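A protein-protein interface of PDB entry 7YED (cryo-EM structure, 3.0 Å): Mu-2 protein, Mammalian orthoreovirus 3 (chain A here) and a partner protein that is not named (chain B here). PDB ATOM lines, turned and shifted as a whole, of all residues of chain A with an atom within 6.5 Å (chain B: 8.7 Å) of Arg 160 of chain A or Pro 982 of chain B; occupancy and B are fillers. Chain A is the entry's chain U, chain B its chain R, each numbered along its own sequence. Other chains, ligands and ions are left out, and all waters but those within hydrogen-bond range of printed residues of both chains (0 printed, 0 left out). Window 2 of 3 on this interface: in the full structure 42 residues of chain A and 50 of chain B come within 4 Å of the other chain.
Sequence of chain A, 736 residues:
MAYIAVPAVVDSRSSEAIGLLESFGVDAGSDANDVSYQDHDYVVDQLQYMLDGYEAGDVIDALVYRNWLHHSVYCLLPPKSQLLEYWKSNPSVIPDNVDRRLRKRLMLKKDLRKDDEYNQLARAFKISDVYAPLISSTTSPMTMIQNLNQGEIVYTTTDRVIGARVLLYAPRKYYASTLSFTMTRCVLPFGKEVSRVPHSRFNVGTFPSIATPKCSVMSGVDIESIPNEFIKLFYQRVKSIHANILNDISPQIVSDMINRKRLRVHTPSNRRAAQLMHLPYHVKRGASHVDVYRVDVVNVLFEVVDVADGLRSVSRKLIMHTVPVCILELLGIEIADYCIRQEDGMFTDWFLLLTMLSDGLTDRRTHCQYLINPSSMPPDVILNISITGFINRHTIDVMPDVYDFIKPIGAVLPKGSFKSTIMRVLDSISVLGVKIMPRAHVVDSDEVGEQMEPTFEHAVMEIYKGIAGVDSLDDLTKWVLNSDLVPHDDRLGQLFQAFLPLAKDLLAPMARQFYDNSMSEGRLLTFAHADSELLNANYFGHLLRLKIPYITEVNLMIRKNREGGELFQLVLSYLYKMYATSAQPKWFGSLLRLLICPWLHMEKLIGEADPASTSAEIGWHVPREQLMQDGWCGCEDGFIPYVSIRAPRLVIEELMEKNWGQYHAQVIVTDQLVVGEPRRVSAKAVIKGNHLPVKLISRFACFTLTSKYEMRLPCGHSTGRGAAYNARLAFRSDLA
Leu 51 of chain A touches Pro 618 of chain B (O to CG, 3.0 Å).
CB of Pro 618 of chain B touches O of Asp 52 of chain A (3.5 Å).
CG of Pro 618 of chain B touches O of Tyr 54 of chain A, at 3.3 Å.
NH2 of Arg 160 of chain A touches CA of Asn 981 of chain B (3.98 Å).
CG of Pro 982 of chain B touches NE of Arg 160 of chain A (3.1 Å).
The side-chain amide oxygen of Asn 981 of chain B lies within hydrogen-bond range of the backbone NH of Leu 984 of chain B (3.2 Å).
O of Pro 982 of chain B lies within hydrogen-bond range of OG of Ser 986 of chain B, at 3.2 Å.
The backbone carbonyl oxygen (O) of Tyr 49 of chain A is in hydrogen-bond range of the guanidinium group (NH1) of Arg 160 of chain A.
NH2 of Arg 160 of chain A is in salt-bridge range of OD2 of Asp 52 of chain A, 3.3 Å away.
Printed residues of chain B within 4 Å of Arg 160 of chain A: Gln 980 (3.1 Å), Asn 981 (3.98 Å) and Pro 982 (3.1 Å).
Of chain A, only Arg 160 (3.1 Å) comes within 4 Å of Pro 982 of chain B.
No residue of chain B comes within 4 Å of Val 161 of chain A.
Of the printed residues of chain B, Tyr 54 of chain A touches Pro 618.
Of the printed residues of chain B, Leu 51 of chain A touches Pro 618.
Val 988 of chain B touches none of the printed residues of chain A.
Met 50 of chain A touches none of the printed residues of chain B.
The side-chain amide oxygen (OE1) of Gln 980 of chain B sits close to the side-chain carboxylate (OD2) of Asp 52 of chain A, at 2.7 Å.
NH2 of Arg 160 of chain A sits at hydrogen-bond distance from O of Gln 980 of chain B.
OD1 of Asp 52 of chain A sits close to O of Gly 621 of chain B (2.9 Å).
Hydrophobic or aromatic side chains of chain B within 4 Å of the printed part of chain A: Pro 618 and Pro 982.
Among the printed residues, 8 pairs touch across the chains.
Among the printed residues, no Asp or Glu carboxylate lies within 4 Å of a Lys or Arg side-chain nitrogen of the other chain.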
ATOM      1  N   GLN A  48      14.329   7.692 -14.678  1.00  0.00           N
ATOM      2  CA  GLN A  48      15.322   6.688 -15.041  1.00  0.00           C
ATOM      3  C   GLN A  48      15.378   6.484 -16.549  1.00  0.00           C
ATOM      4  O   GLN A  48      16.463   6.396 -17.130  1.00  0.00           O
ATOM      5  CB  GLN A  48      15.015   5.368 -14.340  1.00  0.00           C
ATOM      6  CG  GLN A  48      16.037   4.290 -14.616  1.00  0.00           C
ATOM      7  CD  GLN A  48      15.740   3.013 -13.875  1.00  0.00           C
ATOM      8  OE1 GLN A  48      14.738   2.909 -13.169  1.00  0.00           O
ATOM      9  NE2 GLN A  48      16.608   2.025 -14.033  1.00  0.00           N
ATOM     10  N   TYR A  49      14.218   6.410 -17.200  1.00  0.00           N
ATOM     11  CA  TYR A  49      14.202   6.195 -18.643  1.00  0.00           C
ATOM     12  C   TYR A  49      14.717   7.407 -19.403  1.00  0.00           C
ATOM     13  O   TYR A  49      15.243   7.265 -20.511  1.00  0.00           O
ATOM     14  CB  TYR A  49      12.792   5.847 -19.104  1.00  0.00           C
ATOM     15  CG  TYR A  49      12.684   5.590 -20.587  1.00  0.00           C
ATOM     16  CD1 TYR A  49      13.151   4.410 -21.141  1.00  0.00           C
ATOM     17  CD2 TYR A  49      12.112   6.526 -21.432  1.00  0.00           C
ATOM     18  CE1 TYR A  49      13.051   4.172 -22.492  1.00  0.00           C
ATOM     19  CE2 TYR A  49      12.009   6.296 -22.783  1.00  0.00           C
ATOM     20  CZ  TYR A  49      12.480   5.118 -23.309  1.00  0.00           C
ATOM     21  OH  TYR A  49      12.377   4.888 -24.659  1.00  0.00           O
ATOM     22  N   MET A  50      14.577   8.598 -18.832  1.00  0.00           N
ATOM     23  CA  MET A  50      14.943   9.820 -19.529  1.00  0.00           C
ATOM     24  C   MET A  50      16.396  10.198 -19.318  1.00  0.00           C
ATOM     25  O   MET A  50      16.980  10.871 -20.173  1.00  0.00           O
ATOM     26  CB  MET A  50      14.031  10.960 -19.078  1.00  0.00           C
ATOM     27  CG  MET A  50      14.228  12.243 -19.835  1.00  0.00           C
ATOM     28  SD  MET A  50      12.992  13.460 -19.371  1.00  0.00           S
ATOM     29  CE  MET A  50      13.528  14.847 -20.357  1.00  0.00           C
ATOM     30  N   LEU A  51      17.005   9.766 -18.211  1.00  0.00           N
ATOM     31  CA  LEU A  51      18.452   9.886 -18.067  1.00  0.00           C
ATOM     32  C   LEU A  51      19.204   9.025 -19.066  1.00  0.00           C
ATOM     33  O   LEU A  51      20.416   9.202 -19.222  1.00  0.00           O
ATOM     34  CB  LEU A  51      18.890   9.500 -16.655  1.00  0.00           C
ATOM     35  CG  LEU A  51      18.475  10.402 -15.498  1.00  0.00           C
ATOM     36  CD1 LEU A  51      18.898   9.783 -14.180  1.00  0.00           C
ATOM     37  CD2 LEU A  51      19.087  11.769 -15.662  1.00  0.00           C
ATOM     38  N   ASP A  52      18.522   8.093 -19.731  1.00  0.00           N
ATOM     39  CA  ASP A  52      19.178   7.220 -20.692  1.00  0.00           C
ATOM     40  C   ASP A  52      19.589   7.966 -21.953  1.00  0.00           C
ATOM     41  O   ASP A  52      20.615   7.638 -22.557  1.00  0.00           O
ATOM     42  CB  ASP A  52      18.247   6.061 -21.033  1.00  0.00           C
ATOM     43  CG  ASP A  52      18.899   5.037 -21.916  1.00  0.00           C
ATOM     44  OD1 ASP A  52      19.766   4.294 -21.419  1.00  0.00           O
ATOM     45  OD2 ASP A  52      18.536   4.967 -23.107  1.00  0.00           O
ATOM     46  N   GLY A  53      18.811   8.959 -22.373  1.00  0.00           N
ATOM     47  CA  GLY A  53      19.131   9.689 -23.581  1.00  0.00           C
ATOM     48  C   GLY A  53      19.637  11.098 -23.353  1.00  0.00           C
ATOM     49  O   GLY A  53      20.563  11.544 -24.034  1.00  0.00           O
ATOM     50  N   TYR A  54      19.046  11.807 -22.398  1.00  0.00           N
ATOM     51  CA  TYR A  54      19.411  13.188 -22.127  1.00  0.00           C
ATOM     52  C   TYR A  54      20.577  13.236 -21.143  1.00  0.00           C
ATOM     53  O   TYR A  54      21.237  12.232 -20.872  1.00  0.00           O
ATOM     54  CB  TYR A  54      18.219  13.970 -21.587  1.00  0.00           C
ATOM     55  CG  TYR A  54      17.108  14.181 -22.580  1.00  0.00           C
ATOM     56  CD1 TYR A  54      17.188  15.175 -23.541  1.00  0.00           C
ATOM     57  CD2 TYR A  54      15.969  13.393 -22.545  1.00  0.00           C
ATOM     58  CE1 TYR A  54      16.169  15.374 -24.444  1.00  0.00           C
ATOM     59  CE2 TYR A  54      14.946  13.584 -23.440  1.00  0.00           C
ATOM     60  CZ  TYR A  54      15.048  14.573 -24.389  1.00  0.00           C
ATOM     61  OH  TYR A  54      14.023  14.759 -25.284  1.00  0.00           O
ATOM     62  N   ILE A 135       5.568  18.967 -28.236  1.00  0.00           N
ATOM     63  CA  ILE A 135       6.772  19.089 -27.430  1.00  0.00           C
ATOM     64  C   ILE A 135       8.013  19.054 -28.311  1.00  0.00           C
ATOM     65  O   ILE A 135       8.607  20.106 -28.572  1.00  0.00           O
ATOM     66  CB  ILE A 135       6.794  17.986 -26.360  1.00  0.00           C
ATOM     67  CG1 ILE A 135       5.583  18.146 -25.455  1.00  0.00           C
ATOM     68  CG2 ILE A 135       7.984  18.118 -25.486  1.00  0.00           C
ATOM     69  CD1 ILE A 135       5.601  19.453 -24.715  1.00  0.00           C
ATOM     70  N   SER A 137      10.567  15.948 -31.023  1.00  0.00           N
ATOM     71  CA  SER A 137      11.508  14.848 -30.904  1.00  0.00           C
ATOM     72  C   SER A 137      12.840  15.299 -30.318  1.00  0.00           C
ATOM     73  O   SER A 137      13.650  14.452 -29.925  1.00  0.00           O
ATOM     74  CB  SER A 137      11.736  14.192 -32.268  1.00  0.00           C
ATOM     75  OG  SER A 137      10.536  13.622 -32.766  1.00  0.00           O
ATOM     76  N   THR A 138      13.082  16.608 -30.253  1.00  0.00           N
ATOM     77  CA  THR A 138      14.318  17.200 -29.738  1.00  0.00           C
ATOM     78  C   THR A 138      13.987  18.375 -28.825  1.00  0.00           C
ATOM     79  O   THR A 138      14.490  19.487 -28.993  1.00  0.00           O
ATOM     80  CB  THR A 138      15.231  17.654 -30.871  1.00  0.00           C
ATOM     81  OG1 THR A 138      14.571  18.676 -31.627  1.00  0.00           O
ATOM     82  CG2 THR A 138      15.566  16.490 -31.783  1.00  0.00           C
ATOM     83  N   THR A 139      13.109  18.137 -27.849  1.00  0.00           N
ATOM     84  CA  THR A 139      12.488  19.230 -27.107  1.00  0.00           C
ATOM     85  C   THR A 139      13.487  20.045 -26.300  1.00  0.00           C
ATOM     86  O   THR A 139      13.251  21.236 -26.063  1.00  0.00           O
ATOM     87  CB  THR A 139      11.425  18.681 -26.168  1.00  0.00           C
ATOM     88  OG1 THR A 139      10.473  17.924 -26.922  1.00  0.00           O
ATOM     89  CG2 THR A 139      10.722  19.825 -25.461  1.00  0.00           C
ATOM     90  N   MET A 144       9.014  21.384 -21.719  1.00  0.00           N
ATOM     91  CA  MET A 144       8.111  20.326 -21.286  1.00  0.00           C
ATOM     92  C   MET A 144       7.496  20.660 -19.935  1.00  0.00           C
ATOM     93  O   MET A 144       6.271  20.650 -19.771  1.00  0.00           O
ATOM     94  CB  MET A 144       8.867  19.002 -21.219  1.00  0.00           C
ATOM     95  CG  MET A 144       9.374  18.518 -22.556  1.00  0.00           C
ATOM     96  SD  MET A 144      10.338  17.010 -22.416  1.00  0.00           S
ATOM     97  CE  MET A 144       9.054  15.858 -21.970  1.00  0.00           C
ATOM     98  N   THR A 158       6.783  11.795 -28.951  1.00  0.00           N
ATOM     99  CA  THR A 158       7.758  10.831 -28.467  1.00  0.00           C
ATOM    100  C   THR A 158       7.305  10.311 -27.111  1.00  0.00           C
ATOM    101  O   THR A 158       6.295  10.749 -26.558  1.00  0.00           O
ATOM    102  CB  THR A 158       9.156  11.443 -28.353  1.00  0.00           C
ATOM    103  OG1 THR A 158       9.129  12.512 -27.401  1.00  0.00           O
ATOM    104  CG2 THR A 158       9.611  11.976 -29.693  1.00  0.00           C
ATOM    105  N   ASP A 159       8.073   9.366 -26.575  1.00  0.00           N
ATOM    106  CA  ASP A 159       7.763   8.755 -25.292  1.00  0.00           C
ATOM    107  C   ASP A 159       8.611   9.306 -24.160  1.00  0.00           C
ATOM    108  O   ASP A 159       8.166   9.304 -23.008  1.00  0.00           O
ATOM    109  CB  ASP A 159       7.951   7.238 -25.375  1.00  0.00           C
ATOM    110  CG  ASP A 159       7.343   6.507 -24.196  1.00  0.00           C
ATOM    111  OD1 ASP A 159       6.743   7.163 -23.323  1.00  0.00           O
ATOM    112  OD2 ASP A 159       7.469   5.265 -24.138  1.00  0.00           O
ATOM    113  N   ARG A 160       9.802   9.811 -24.461  1.00  0.00           N
ATOM    114  CA  ARG A 160      10.676  10.330 -23.420  1.00  0.00           C
ATOM    115  C   ARG A 160      10.121  11.641 -22.891  1.00  0.00           C
ATOM    116  O   ARG A 160      10.461  12.718 -23.389  1.00  0.00           O
ATOM    117  CB  ARG A 160      12.095  10.531 -23.946  1.00  0.00           C
ATOM    118  CG  ARG A 160      12.822   9.250 -24.281  1.00  0.00           C
ATOM    119  CD  ARG A 160      14.237   9.528 -24.733  1.00  0.00           C
ATOM    120  NE  ARG A 160      14.905   8.308 -25.167  1.00  0.00           N
ATOM    121  CZ  ARG A 160      15.576   7.497 -24.358  1.00  0.00           C
ATOM    122  NH1 ARG A 160      15.669   7.778 -23.068  1.00  0.00           N
ATOM    123  NH2 ARG A 160      16.153   6.406 -24.841  1.00  0.00           N
ATOM    124  N   VAL A 161       9.253  11.551 -21.888  1.00  0.00           N
ATOM    125  CA  VAL A 161       8.667  12.717 -21.249  1.00  0.00           C
ATOM    126  C   VAL A 161       8.601  12.445 -19.756  1.00  0.00           C
ATOM    127  O   VAL A 161       8.618  11.297 -19.308  1.00  0.00           O
ATOM    128  CB  VAL A 161       7.270  13.044 -21.804  1.00  0.00           C
ATOM    129  CG1 VAL A 161       7.359  13.361 -23.281  1.00  0.00           C
ATOM    130  CG2 VAL A 161       6.338  11.881 -21.569  1.00  0.00           C
ATOM    131  N   ILE A 162       8.526  13.520 -18.982  1.00  0.00           N
ATOM    132  CA  ILE A 162       8.608  13.425 -17.531  1.00  0.00           C
ATOM    133  C   ILE A 162       7.762  14.534 -16.932  1.00  0.00           C
ATOM    134  O   ILE A 162       7.750  15.659 -17.433  1.00  0.00           O
ATOM    135  CB  ILE A 162      10.070  13.510 -17.055  1.00  0.00           C
ATOM    136  CG1 ILE A 162      10.181  13.165 -15.574  1.00  0.00           C
ATOM    137  CG2 ILE A 162      10.631  14.889 -17.320  1.00  0.00           C
ATOM    138  CD1 ILE A 162      11.596  12.929 -15.126  1.00  0.00           C
ATOM    139  N   PRO B 445      25.535   8.633 -31.463  1.00  0.00           N
ATOM    140  CA  PRO B 445      24.728   7.412 -31.368  1.00  0.00           C
ATOM    141  C   PRO B 445      25.217   6.298 -32.269  1.00  0.00           C
ATOM    142  O   PRO B 445      24.972   5.125 -31.967  1.00  0.00           O
ATOM    143  CB  PRO B 445      23.328   7.888 -31.771  1.00  0.00           C
ATOM    144  CG  PRO B 445      23.333   9.347 -31.503  1.00  0.00           C
ATOM    145  CD  PRO B 445      24.722   9.804 -31.825  1.00  0.00           C
ATOM    146  N   PRO B 618      25.346   9.768 -20.615  1.00  0.00           N
ATOM    147  CA  PRO B 618      25.162   8.315 -20.658  1.00  0.00           C
ATOM    148  C   PRO B 618      25.945   7.663 -21.784  1.00  0.00           C
ATOM    149  O   PRO B 618      26.069   8.192 -22.890  1.00  0.00           O
ATOM    150  CB  PRO B 618      23.654   8.165 -20.901  1.00  0.00           C
ATOM    151  CG  PRO B 618      23.064   9.478 -20.527  1.00  0.00           C
ATOM    152  CD  PRO B 618      24.099  10.478 -20.925  1.00  0.00           C
ATOM    153  N   GLY B 621      23.343   3.171 -23.391  1.00  0.00           N
ATOM    154  CA  GLY B 621      22.103   2.854 -22.714  1.00  0.00           C
ATOM    155  C   GLY B 621      22.236   2.685 -21.222  1.00  0.00           C
ATOM    156  O   GLY B 621      21.421   1.990 -20.611  1.00  0.00           O
ATOM    157  N   ASP B 976      13.686  -2.112 -31.702  1.00  0.00           N
ATOM    158  CA  ASP B 976      13.703  -1.239 -30.534  1.00  0.00           C
ATOM    159  C   ASP B 976      15.021  -1.361 -29.786  1.00  0.00           C
ATOM    160  O   ASP B 976      15.549  -0.367 -29.273  1.00  0.00           O
ATOM    161  CB  ASP B 976      12.530  -1.581 -29.620  1.00  0.00           C
ATOM    162  CG  ASP B 976      12.345  -0.581 -28.501  1.00  0.00           C
ATOM    163  OD1 ASP B 976      13.123   0.389 -28.417  1.00  0.00           O
ATOM    164  OD2 ASP B 976      11.410  -0.770 -27.696  1.00  0.00           O
ATOM    165  N   MET B 979      17.851   0.669 -32.309  1.00  0.00           N
ATOM    166  CA  MET B 979      17.741   2.128 -32.265  1.00  0.00           C
ATOM    167  C   MET B 979      17.064   2.509 -30.953  1.00  0.00           C
ATOM    168  O   MET B 979      15.848   2.672 -30.885  1.00  0.00           O
ATOM    169  CB  MET B 979      16.961   2.651 -33.465  1.00  0.00           C
ATOM    170  CG  MET B 979      17.651   2.437 -34.797  1.00  0.00           C
ATOM    171  SD  MET B 979      16.712   3.133 -36.165  1.00  0.00           S
ATOM    172  CE  MET B 979      15.367   1.958 -36.282  1.00  0.00           C
ATOM    173  N   GLN B 980      17.868   2.668 -29.903  1.00  0.00           N
ATOM    174  CA  GLN B 980      17.324   2.921 -28.577  1.00  0.00           C
ATOM    175  C   GLN B 980      17.212   4.401 -28.241  1.00  0.00           C
ATOM    176  O   GLN B 980      16.282   4.793 -27.528  1.00  0.00           O
ATOM    177  CB  GLN B 980      18.169   2.208 -27.515  1.00  0.00           C
ATOM    178  CG  GLN B 980      19.625   2.654 -27.424  1.00  0.00           C
ATOM    179  CD  GLN B 980      19.828   3.820 -26.475  1.00  0.00           C
ATOM    180  OE1 GLN B 980      19.087   3.980 -25.508  1.00  0.00           O
ATOM    181  NE2 GLN B 980      20.835   4.641 -26.750  1.00  0.00           N
ATOM    182  N   ASN B 981      18.122   5.232 -28.724  1.00  0.00           N
ATOM    183  CA  ASN B 981      18.054   6.629 -28.333  1.00  0.00           C
ATOM    184  C   ASN B 981      17.331   7.463 -29.377  1.00  0.00           C
ATOM    185  O   ASN B 981      17.233   7.078 -30.545  1.00  0.00           O
ATOM    186  CB  ASN B 981      19.457   7.195 -28.094  1.00  0.00           C
ATOM    187  CG  ASN B 981      20.343   7.124 -29.322  1.00  0.00           C
ATOM    188  OD1 ASN B 981      19.917   6.716 -30.402  1.00  0.00           O
ATOM    189  ND2 ASN B 981      21.592   7.533 -29.160  1.00  0.00           N
ATOM    190  N   PRO B 982      16.814   8.628 -28.984  1.00  0.00           N
ATOM    191  CA  PRO B 982      16.052   9.450 -29.936  1.00  0.00           C
ATOM    192  C   PRO B 982      16.873   9.962 -31.102  1.00  0.00           C
ATOM    193  O   PRO B 982      16.295  10.307 -32.136  1.00  0.00           O
ATOM    194  CB  PRO B 982      15.546  10.611 -29.067  1.00  0.00           C
ATOM    195  CG  PRO B 982      15.580  10.086 -27.675  1.00  0.00           C
ATOM    196  CD  PRO B 982      16.766   9.174 -27.619  1.00  0.00           C
ATOM    197  N   GLU B 983      18.200  10.019 -30.979  1.00  0.00           N
ATOM    198  CA  GLU B 983      18.999  10.654 -32.020  1.00  0.00           C
ATOM    199  C   GLU B 983      19.124   9.765 -33.253  1.00  0.00           C
ATOM    200  O   GLU B 983      18.978  10.246 -34.383  1.00  0.00           O
ATOM    201  CB  GLU B 983      20.370  11.035 -31.461  1.00  0.00           C
ATOM    202  CG  GLU B 983      20.283  12.132 -30.406  1.00  0.00           C
ATOM    203  CD  GLU B 983      21.632  12.543 -29.846  1.00  0.00           C
ATOM    204  OE1 GLU B 983      22.646  11.895 -30.177  1.00  0.00           O
ATOM    205  OE2 GLU B 983      21.678  13.522 -29.072  1.00  0.00           O
ATOM    206  N   LEU B 984      19.389   8.468 -33.066  1.00  0.00           N
ATOM    207  CA  LEU B 984      19.414   7.554 -34.205  1.00  0.00           C
ATOM    208  C   LEU B 984      18.064   7.516 -34.906  1.00  0.00           C
ATOM    209  O   LEU B 984      17.991   7.549 -36.144  1.00  0.00           O
ATOM    210  CB  LEU B 984      19.801   6.147 -33.756  1.00  0.00           C
ATOM    211  CG  LEU B 984      21.223   5.889 -33.282  1.00  0.00           C
ATOM    212  CD1 LEU B 984      21.338   4.476 -32.748  1.00  0.00           C
ATOM    213  CD2 LEU B 984      22.189   6.102 -34.423  1.00  0.00           C
ATOM    214  N   LYS B 985      16.985   7.432 -34.127  1.00  0.00           N
ATOM    215  CA  LYS B 985      15.651   7.390 -34.709  1.00  0.00           C
ATOM    216  C   LYS B 985      15.343   8.671 -35.467  1.00  0.00           C
ATOM    217  O   LYS B 985      14.766   8.632 -36.558  1.00  0.00           O
ATOM    218  CB  LYS B 985      14.613   7.147 -33.615  1.00  0.00           C
ATOM    219  CG  LYS B 985      13.206   6.938 -34.136  1.00  0.00           C
ATOM    220  CD  LYS B 985      12.238   6.679 -32.999  1.00  0.00           C
ATOM    221  CE  LYS B 985      12.476   5.313 -32.382  1.00  0.00           C
ATOM    222  NZ  LYS B 985      12.139   4.212 -33.324  1.00  0.00           N
ATOM    223  N   SER B 986      15.735   9.819 -34.912  1.00  0.00           N
ATOM    224  CA  SER B 986      15.505  11.086 -35.595  1.00  0.00           C
ATOM    225  C   SER B 986      16.289  11.154 -36.896  1.00  0.00           C
ATOM    226  O   SER B 986      15.764  11.607 -37.921  1.00  0.00           O
ATOM    227  CB  SER B 986      15.880  12.248 -34.679  1.00  0.00           C
ATOM    228  OG  SER B 986      17.273  12.251 -34.423  1.00  0.00           O
ATOM    229  N   ARG B 987      17.544  10.698 -36.878  1.00  0.00           N
ATOM    230  CA  ARG B 987      18.349  10.686 -38.096  1.00  0.00           C
ATOM    231  C   ARG B 987      17.694   9.833 -39.174  1.00  0.00           C
ATOM    232  O   ARG B 987      17.533  10.272 -40.318  1.00  0.00           O
ATOM    233  CB  ARG B 987      19.756  10.173 -37.791  1.00  0.00           C
ATOM    234  CG  ARG B 987      20.583  11.099 -36.923  1.00  0.00           C
ATOM    235  CD  ARG B 987      21.960  10.518 -36.666  1.00  0.00           C
ATOM    236  NE  ARG B 987      22.758  11.380 -35.802  1.00  0.00           N
ATOM    237  CZ  ARG B 987      23.983  11.086 -35.383  1.00  0.00           C
ATOM    238  NH1 ARG B 987      24.556   9.948 -35.749  1.00  0.00           N
ATOM    239  NH2 ARG B 987      24.637  11.928 -34.598  1.00  0.00           N
ATOM    240  N   VAL B 988      17.285   8.615 -38.818  1.00  0.00           N
ATOM    241  CA  VAL B 988      16.754   7.709 -39.832  1.00  0.00           C
ATOM    242  C   VAL B 988      15.392   8.186 -40.325  1.00  0.00           C
ATOM    243  O   VAL B 988      15.067   8.058 -41.512  1.00  0.00           O
ATOM    244  CB  VAL B 988      16.697   6.273 -39.288  1.00  0.00           C
ATOM    245  CG1 VAL B 988      16.151   5.338 -40.342  1.00  0.00           C
ATOM    246  CG2 VAL B 988      18.075   5.821 -38.850  1.00  0.00           C
ATOM    247  N   LEU B 989      14.579   8.762 -39.436  1.00  0.00           N
ATOM    248  CA  LEU B 989      13.273   9.257 -39.858  1.00  0.00           C
ATOM    249  C   LEU B 989      13.413  10.472 -40.769  1.00  0.00           C
ATOM    250  O   LEU B 989      12.686  10.593 -41.764  1.00  0.00           O
ATOM    251  CB  LEU B 989      12.417   9.589 -38.638  1.00  0.00           C
ATOM    252  CG  LEU B 989      12.022   8.401 -37.759  1.00  0.00           C
ATOM    253  CD1 LEU B 989      11.289   8.871 -36.517  1.00  0.00           C
ATOM    254  CD2 LEU B 989      11.175   7.413 -38.539  1.00  0.00           C
ATOM    255  N   ARG B 990      14.333  11.384 -40.444  1.00  0.00           N
ATOM    256  CA  ARG B 990      14.598  12.506 -41.334  1.00  0.00           C
ATOM    257  C   ARG B 990      15.113  12.021 -42.681  1.00  0.00           C
ATOM    258  O   ARG B 990      14.753  12.575 -43.728  1.00  0.00           O
ATOM    259  CB  ARG B 990      15.599  13.461 -40.689  1.00  0.00           C
ATOM    260  CG  ARG B 990      15.903  14.690 -41.518  1.00  0.00           C
ATOM    261  CD  ARG B 990      16.841  15.623 -40.780  1.00  0.00           C
ATOM    262  NE  ARG B 990      16.204  16.203 -39.603  1.00  0.00           N
ATOM    263  CZ  ARG B 990      16.842  16.921 -38.685  1.00  0.00           C
ATOM    264  NH1 ARG B 990      18.141  17.150 -38.805  1.00  0.00           N
ATOM    265  NH2 ARG B 990      16.178  17.408 -37.646  1.00  0.00           N
